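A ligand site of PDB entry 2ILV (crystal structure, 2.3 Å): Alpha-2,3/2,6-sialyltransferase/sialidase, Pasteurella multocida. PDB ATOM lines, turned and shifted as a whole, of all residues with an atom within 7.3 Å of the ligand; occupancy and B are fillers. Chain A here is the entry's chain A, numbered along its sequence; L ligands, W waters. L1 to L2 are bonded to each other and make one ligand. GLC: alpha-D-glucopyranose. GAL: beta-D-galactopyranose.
Residues that only touch the ligand: Pro 11, Ala 12 and Arg 40. Of the 22 residues printed, 8 come within 4 Å of the ligand. Along chain A the residues within 4 Å of the ligand span positions 11 to 247. The nearest printed residue that does not touch the ligand is Asn 86 (4.1 Å).
The side-chain carboxylate (OD2) of Asp 118 sits at hydrogen-bond distance from an oxygen (O3) of GAL L2, at 2.5 Å. A ring nitrogen (NE2) of His 89 lies within hydrogen-bond range of an oxygen (O4) of GAL L2 (2.8 Å). The side-chain amide oxygen (OD1) of Asn 62 sits at hydrogen-bond distance from an oxygen (O6) of GAL L2 (2.9 Å). The indole nitrogen (NE1) of Trp 247 is in hydrogen-bond range of an oxygen (O2) of GAL L2, at 3.1 Å. The side-chain sulfur (SD) of Met 121 lies within hydrogen-bond range of an oxygen (O2) of GAL L2, 3.6 Å away.
ND2 of Asn 86 sits at hydrogen-bond distance from OD1 of Asp 118 (2.7 Å). OE2 of Glu 122 is in hydrogen-bond range of N of Asp 118 (2.7 Å). The backbone NH of His 89 lies within hydrogen-bond range of the side-chain amide oxygen of Asn 86, 3.2 Å away. The backbone NH of Ala 12 lies within hydrogen-bond range of the side-chain carboxylate of Asp 10 (2.7 Å). O of Pro 11 lies within hydrogen-bond range of NE of Arg 40 (3.3 Å). The guanidinium group (NH1) of Arg 40 lies within hydrogen-bond range of the side-chain hydroxyl (OG) of Ser 13 (2.6 Å).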
ATOM      1  N   ASP A  10      26.893 -13.086 -37.146  1.00  0.00           N
ATOM      2  CA  ASP A  10      26.460 -13.628 -35.879  1.00  0.00           C
ATOM      3  C   ASP A  10      26.384 -15.148 -35.967  1.00  0.00           C
ATOM      4  O   ASP A  10      25.676 -15.692 -36.828  1.00  0.00           O
ATOM      5  CB  ASP A  10      25.082 -13.082 -35.506  1.00  0.00           C
ATOM      6  CG  ASP A  10      24.633 -13.534 -34.149  1.00  0.00           C
ATOM      7  OD1 ASP A  10      25.466 -14.029 -33.358  1.00  0.00           O
ATOM      8  OD2 ASP A  10      23.428 -13.387 -33.857  1.00  0.00           O
ATOM      9  N   PRO A  11      27.142 -15.840 -35.079  1.00  0.00           N
ATOM     10  CA  PRO A  11      26.969 -17.290 -34.923  1.00  0.00           C
ATOM     11  C   PRO A  11      25.802 -17.707 -34.009  1.00  0.00           C
ATOM     12  O   PRO A  11      25.404 -18.892 -34.010  1.00  0.00           O
ATOM     13  CB  PRO A  11      28.304 -17.734 -34.332  1.00  0.00           C
ATOM     14  CG  PRO A  11      28.831 -16.512 -33.582  1.00  0.00           C
ATOM     15  CD  PRO A  11      28.217 -15.301 -34.206  1.00  0.00           C
ATOM     16  N   ALA A  12      25.247 -16.758 -33.264  1.00  0.00           N
ATOM     17  CA  ALA A  12      24.158 -17.017 -32.320  1.00  0.00           C
ATOM     18  C   ALA A  12      22.816 -16.512 -32.827  1.00  0.00           C
ATOM     19  O   ALA A  12      22.543 -16.613 -34.025  1.00  0.00           O
ATOM     20  CB  ALA A  12      24.497 -16.456 -30.929  1.00  0.00           C
ATOM     21  N   SER A  13      21.953 -15.986 -31.948  1.00  0.00           N
ATOM     22  CA  SER A  13      20.525 -15.790 -32.290  1.00  0.00           C
ATOM     23  C   SER A  13      20.111 -14.345 -32.160  1.00  0.00           C
ATOM     24  O   SER A  13      19.645 -13.744 -33.102  1.00  0.00           O
ATOM     25  CB  SER A  13      19.597 -16.626 -31.374  1.00  0.00           C
ATOM     26  OG  SER A  13      19.933 -18.000 -31.371  1.00  0.00           O
ATOM     27  N   PRO A  15      21.769 -11.332 -31.732  1.00  0.00           N
ATOM     28  CA  PRO A  15      22.279 -10.363 -32.723  1.00  0.00           C
ATOM     29  C   PRO A  15      21.700 -10.539 -34.145  1.00  0.00           C
ATOM     30  O   PRO A  15      21.356  -9.550 -34.773  1.00  0.00           O
ATOM     31  CB  PRO A  15      23.808 -10.597 -32.716  1.00  0.00           C
ATOM     32  CG  PRO A  15      24.081 -11.321 -31.437  1.00  0.00           C
ATOM     33  CD  PRO A  15      22.855 -12.132 -31.133  1.00  0.00           C
ATOM     34  N   SER A  39      24.751 -17.859 -38.803  1.00  0.00           N
ATOM     35  CA  SER A  39      24.791 -19.319 -38.688  1.00  0.00           C
ATOM     36  C   SER A  39      23.403 -19.919 -38.484  1.00  0.00           C
ATOM     37  O   SER A  39      23.093 -20.988 -39.019  1.00  0.00           O
ATOM     38  CB  SER A  39      25.705 -19.744 -37.530  1.00  0.00           C
ATOM     39  OG  SER A  39      27.015 -19.230 -37.656  1.00  0.00           O
ATOM     40  N   ARG A  40      22.580 -19.235 -37.705  1.00  0.00           N
ATOM     41  CA  ARG A  40      21.289 -19.783 -37.324  1.00  0.00           C
ATOM     42  C   ARG A  40      20.113 -19.336 -38.226  1.00  0.00           C
ATOM     43  O   ARG A  40      18.955 -19.635 -37.896  1.00  0.00           O
ATOM     44  CB  ARG A  40      21.025 -19.486 -35.838  1.00  0.00           C
ATOM     45  CG  ARG A  40      22.017 -20.188 -34.893  1.00  0.00           C
ATOM     46  CD  ARG A  40      21.600 -20.128 -33.391  1.00  0.00           C
ATOM     47  NE  ARG A  40      22.767 -20.265 -32.502  1.00  0.00           N
ATOM     48  CZ  ARG A  40      22.768 -20.057 -31.180  1.00  0.00           C
ATOM     49  NH1 ARG A  40      21.662 -19.688 -30.527  1.00  0.00           N
ATOM     50  NH2 ARG A  40      23.892 -20.213 -30.501  1.00  0.00           N
ATOM     51  N   ASP A  61      34.486 -21.454 -35.931  1.00  0.00           N
ATOM     52  CA  ASP A  61      35.214 -20.980 -34.753  1.00  0.00           C
ATOM     53  C   ASP A  61      34.934 -19.498 -34.471  1.00  0.00           C
ATOM     54  O   ASP A  61      35.836 -18.750 -34.121  1.00  0.00           O
ATOM     55  CB  ASP A  61      36.728 -21.265 -34.881  1.00  0.00           C
ATOM     56  CG  ASP A  61      37.021 -22.736 -35.149  1.00  0.00           C
ATOM     57  OD1 ASP A  61      36.593 -23.567 -34.339  1.00  0.00           O
ATOM     58  OD2 ASP A  61      37.635 -23.064 -36.179  1.00  0.00           O
ATOM     59  N   ASN A  62      33.663 -19.107 -34.612  1.00  0.00           N
ATOM     60  CA  ASN A  62      33.147 -17.742 -34.329  1.00  0.00           C
ATOM     61  C   ASN A  62      33.657 -16.633 -35.237  1.00  0.00           C
ATOM     62  O   ASN A  62      33.855 -15.515 -34.767  1.00  0.00           O
ATOM     63  CB  ASN A  62      33.445 -17.334 -32.886  1.00  0.00           C
ATOM     64  CG  ASN A  62      32.812 -18.252 -31.870  1.00  0.00           C
ATOM     65  OD1 ASN A  62      31.623 -18.561 -31.964  1.00  0.00           O
ATOM     66  ND2 ASN A  62      33.590 -18.667 -30.879  1.00  0.00           N
ATOM     67  N   ASN A  86      28.000  -9.643 -33.229  1.00  0.00           N
ATOM     68  CA  ASN A  86      27.907 -10.171 -31.878  1.00  0.00           C
ATOM     69  C   ASN A  86      28.974  -9.555 -30.950  1.00  0.00           C
ATOM     70  O   ASN A  86      30.194  -9.673 -31.215  1.00  0.00           O
ATOM     71  CB  ASN A  86      28.124 -11.684 -31.970  1.00  0.00           C
ATOM     72  CG  ASN A  86      27.805 -12.399 -30.682  1.00  0.00           C
ATOM     73  OD1 ASN A  86      28.331 -12.088 -29.604  1.00  0.00           O
ATOM     74  ND2 ASN A  86      26.946 -13.389 -30.787  1.00  0.00           N
ATOM     75  N   ALA A  88      29.945 -10.407 -27.739  1.00  0.00           N
ATOM     76  CA  ALA A  88      30.807 -11.368 -27.076  1.00  0.00           C
ATOM     77  C   ALA A  88      31.901 -11.898 -28.013  1.00  0.00           C
ATOM     78  O   ALA A  88      33.045 -12.139 -27.576  1.00  0.00           O
ATOM     79  CB  ALA A  88      29.974 -12.530 -26.484  1.00  0.00           C
ATOM     80  N   HIS A  89      31.553 -12.096 -29.298  1.00  0.00           N
ATOM     81  CA  HIS A  89      32.482 -12.636 -30.310  1.00  0.00           C
ATOM     82  C   HIS A  89      33.102 -11.590 -31.257  1.00  0.00           C
ATOM     83  O   HIS A  89      33.722 -11.957 -32.237  1.00  0.00           O
ATOM     84  CB  HIS A  89      31.775 -13.716 -31.166  1.00  0.00           C
ATOM     85  CG  HIS A  89      31.131 -14.785 -30.348  1.00  0.00           C
ATOM     86  ND1 HIS A  89      31.850 -15.794 -29.742  1.00  0.00           N
ATOM     87  CD2 HIS A  89      29.832 -14.999 -30.039  1.00  0.00           C
ATOM     88  CE1 HIS A  89      31.031 -16.577 -29.075  1.00  0.00           C
ATOM     89  NE2 HIS A  89      29.802 -16.113 -29.238  1.00  0.00           N
ATOM     90  N   ASP A 118      25.049 -10.860 -27.489  1.00  0.00           N
ATOM     91  CA  ASP A 118      24.850 -12.264 -27.697  1.00  0.00           C
ATOM     92  C   ASP A 118      23.635 -12.647 -26.838  1.00  0.00           C
ATOM     93  O   ASP A 118      22.791 -13.483 -27.225  1.00  0.00           O
ATOM     94  CB  ASP A 118      26.110 -13.002 -27.227  1.00  0.00           C
ATOM     95  CG  ASP A 118      26.048 -14.495 -27.472  1.00  0.00           C
ATOM     96  OD1 ASP A 118      26.136 -14.889 -28.648  1.00  0.00           O
ATOM     97  OD2 ASP A 118      25.887 -15.258 -26.496  1.00  0.00           O
ATOM     98  N   GLY A 119      23.568 -12.011 -25.666  1.00  0.00           N
ATOM     99  CA  GLY A 119      22.535 -12.289 -24.666  1.00  0.00           C
ATOM    100  C   GLY A 119      23.011 -12.115 -23.240  1.00  0.00           C
ATOM    101  O   GLY A 119      23.672 -11.130 -22.930  1.00  0.00           O
ATOM    102  N   SER A 120      22.612 -13.055 -22.374  1.00  0.00           N
ATOM    103  CA  SER A 120      23.111 -13.173 -20.971  1.00  0.00           C
ATOM    104  C   SER A 120      24.637 -13.292 -20.863  1.00  0.00           C
ATOM    105  O   SER A 120      25.237 -12.768 -19.910  1.00  0.00           O
ATOM    106  CB  SER A 120      22.468 -14.393 -20.257  1.00  0.00           C
ATOM    107  OG  SER A 120      22.781 -15.627 -20.897  1.00  0.00           O
ATOM    108  N   MET A 121      25.263 -13.960 -21.825  1.00  0.00           N
ATOM    109  CA  MET A 121      26.713 -14.201 -21.744  1.00  0.00           C
ATOM    110  C   MET A 121      27.534 -12.934 -21.437  1.00  0.00           C
ATOM    111  O   MET A 121      28.466 -12.993 -20.656  1.00  0.00           O
ATOM    112  CB  MET A 121      27.232 -14.886 -23.015  1.00  0.00           C
ATOM    113  CG  MET A 121      28.758 -15.057 -23.051  1.00  0.00           C
ATOM    114  SD  MET A 121      29.316 -16.337 -24.208  1.00  0.00           S
ATOM    115  CE  MET A 121      28.948 -15.544 -25.739  1.00  0.00           C
ATOM    116  N   GLU A 122      27.213 -11.811 -22.098  1.00  0.00           N
ATOM    117  CA  GLU A 122      27.876 -10.537 -21.865  1.00  0.00           C
ATOM    118  C   GLU A 122      27.760 -10.076 -20.425  1.00  0.00           C
ATOM    119  O   GLU A 122      28.722  -9.563 -19.871  1.00  0.00           O
ATOM    120  CB  GLU A 122      27.277  -9.463 -22.772  1.00  0.00           C
ATOM    121  CG  GLU A 122      27.897  -9.389 -24.143  1.00  0.00           C
ATOM    122  CD  GLU A 122      27.268 -10.382 -25.101  1.00  0.00           C
ATOM    123  OE1 GLU A 122      26.603 -11.330 -24.641  1.00  0.00           O
ATOM    124  OE2 GLU A 122      27.423 -10.192 -26.326  1.00  0.00           O
ATOM    125  N   TRP A 247      26.879 -25.969 -24.528  1.00  0.00           N
ATOM    126  CA  TRP A 247      27.965 -25.712 -25.513  1.00  0.00           C
ATOM    127  C   TRP A 247      29.135 -26.705 -25.361  1.00  0.00           C
ATOM    128  O   TRP A 247      30.296 -26.337 -25.492  1.00  0.00           O
ATOM    129  CB  TRP A 247      28.464 -24.239 -25.466  1.00  0.00           C
ATOM    130  CG  TRP A 247      27.340 -23.284 -25.581  1.00  0.00           C
ATOM    131  CD1 TRP A 247      26.801 -22.520 -24.581  1.00  0.00           C
ATOM    132  CD2 TRP A 247      26.547 -23.031 -26.755  1.00  0.00           C
ATOM    133  NE1 TRP A 247      25.725 -21.794 -25.053  1.00  0.00           N
ATOM    134  CE2 TRP A 247      25.554 -22.093 -26.383  1.00  0.00           C
ATOM    135  CE3 TRP A 247      26.582 -23.509 -28.065  1.00  0.00           C
ATOM    136  CZ2 TRP A 247      24.611 -21.605 -27.294  1.00  0.00           C
ATOM    137  CZ3 TRP A 247      25.640 -23.034 -28.973  1.00  0.00           C
ATOM    138  CH2 TRP A 247      24.671 -22.097 -28.581  1.00  0.00           C
ATOM    139  N   GLU A 248      28.787 -27.959 -25.085  1.00  0.00           N
ATOM    140  CA  GLU A 248      29.746 -29.035 -24.883  1.00  0.00           C
ATOM    141  C   GLU A 248      29.259 -30.198 -25.717  1.00  0.00           C
ATOM    142  O   GLU A 248      28.156 -30.703 -25.464  1.00  0.00           O
ATOM    143  CB  GLU A 248      29.766 -29.468 -23.409  1.00  0.00           C
ATOM    144  CG  GLU A 248      30.184 -28.417 -22.384  1.00  0.00           C
ATOM    145  CD  GLU A 248      30.037 -28.932 -20.951  1.00  0.00           C
ATOM    146  OE1 GLU A 248      29.266 -28.338 -20.172  1.00  0.00           O
ATOM    147  OE2 GLU A 248      30.701 -29.949 -20.604  1.00  0.00           O
ATOM    148  N   HIS A 288      15.491 -24.574 -27.303  1.00  0.00           N
ATOM    149  CA  HIS A 288      16.640 -23.752 -27.688  1.00  0.00           C
ATOM    150  C   HIS A 288      16.907 -24.025 -29.168  1.00  0.00           C
ATOM    151  O   HIS A 288      16.837 -25.177 -29.583  1.00  0.00           O
ATOM    152  CB  HIS A 288      17.873 -24.104 -26.851  1.00  0.00           C
ATOM    153  CG  HIS A 288      18.917 -23.041 -26.903  1.00  0.00           C
ATOM    154  ND1 HIS A 288      19.785 -22.903 -27.972  1.00  0.00           N
ATOM    155  CD2 HIS A 288      19.197 -22.032 -26.045  1.00  0.00           C
ATOM    156  CE1 HIS A 288      20.567 -21.853 -27.755  1.00  0.00           C
ATOM    157  NE2 HIS A 288      20.224 -21.301 -26.606  1.00  0.00           N
ATOM    158  N   ARG A 290      19.556 -24.384 -30.742  1.00  0.00           N
ATOM    159  CA  ARG A 290      20.650 -25.345 -30.890  1.00  0.00           C
ATOM    160  C   ARG A 290      20.462 -26.536 -29.965  1.00  0.00           C
ATOM    161  O   ARG A 290      21.375 -27.346 -29.821  1.00  0.00           O
ATOM    162  CB  ARG A 290      22.001 -24.700 -30.615  1.00  0.00           C
ATOM    163  CG  ARG A 290      22.416 -23.573 -31.567  1.00  0.00           C
ATOM    164  CD  ARG A 290      22.276 -23.893 -33.047  1.00  0.00           C
ATOM    165  NE  ARG A 290      22.992 -25.087 -33.511  1.00  0.00           N
ATOM    166  CZ  ARG A 290      24.297 -25.328 -33.361  1.00  0.00           C
ATOM    167  NH1 ARG A 290      25.091 -24.472 -32.714  1.00  0.00           N
ATOM    168  NH2 ARG A 290      24.823 -26.440 -33.863  1.00  0.00           N
ATOM    169  N   SER A 333      18.488 -15.863 -22.160  1.00  0.00           N
ATOM    170  CA  SER A 333      18.514 -14.460 -22.648  1.00  0.00           C
ATOM    171  C   SER A 333      17.106 -13.884 -22.953  1.00  0.00           C
ATOM    172  O   SER A 333      16.892 -12.652 -22.895  1.00  0.00           O
ATOM    173  CB  SER A 333      19.326 -14.371 -23.931  1.00  0.00           C
ATOM    174  OG  SER A 333      20.633 -14.919 -23.755  1.00  0.00           O
HETATM  175  C1  GLC L   1      33.424 -21.665 -25.874  1.00  0.00           C
HETATM  176  C2  GLC L   1      32.987 -21.464 -27.323  1.00  0.00           C
HETATM  177  C3  GLC L   1      31.968 -20.338 -27.468  1.00  0.00           C
HETATM  178  C4  GLC L   1      30.804 -20.544 -26.482  1.00  0.00           C
HETATM  179  C5  GLC L   1      31.356 -20.734 -25.064  1.00  0.00           C
HETATM  180  C6  GLC L   1      30.270 -20.947 -24.005  1.00  0.00           C
HETATM  181  O1  GLC L   1      34.133 -20.511 -25.430  1.00  0.00           O
HETATM  182  O2  GLC L   1      34.109 -21.180 -28.159  1.00  0.00           O
HETATM  183  O3  GLC L   1      31.498 -20.309 -28.826  1.00  0.00           O
HETATM  184  O4  GLC L   1      29.917 -19.445 -26.538  1.00  0.00           O
HETATM  185  O5  GLC L   1      32.271 -21.837 -25.041  1.00  0.00           O
HETATM  186  O6  GLC L   1      30.886 -20.975 -22.717  1.00  0.00           O
HETATM  187  C1  GAL L   2      28.687 -19.687 -27.232  1.00  0.00           C
HETATM  188  C2  GAL L   2      27.649 -18.748 -26.627  1.00  0.00           C
HETATM  189  C3  GAL L   2      26.361 -18.705 -27.459  1.00  0.00           C
HETATM  190  C4  GAL L   2      26.685 -18.502 -28.945  1.00  0.00           C
HETATM  191  C5  GAL L   2      27.704 -19.540 -29.424  1.00  0.00           C
HETATM  192  C6  GAL L   2      28.008 -19.423 -30.930  1.00  0.00           C
HETATM  193  O2  GAL L   2      27.405 -19.165 -25.267  1.00  0.00           O
HETATM  194  O3  GAL L   2      25.467 -17.670 -26.980  1.00  0.00           O
HETATM  195  O4  GAL L   2      27.230 -17.201 -29.184  1.00  0.00           O
HETATM  196  O5  GAL L   2      28.890 -19.416 -28.614  1.00  0.00           O
HETATM  197  O6  GAL L   2      29.227 -20.111 -31.218  1.00  0.00           O
HETATM  198  O   HOH W   1      28.084 -21.892 -32.731  1.00  0.00           O
HETATM  199  O   HOH W   2      30.523 -23.247 -29.558  1.00  0.00           O
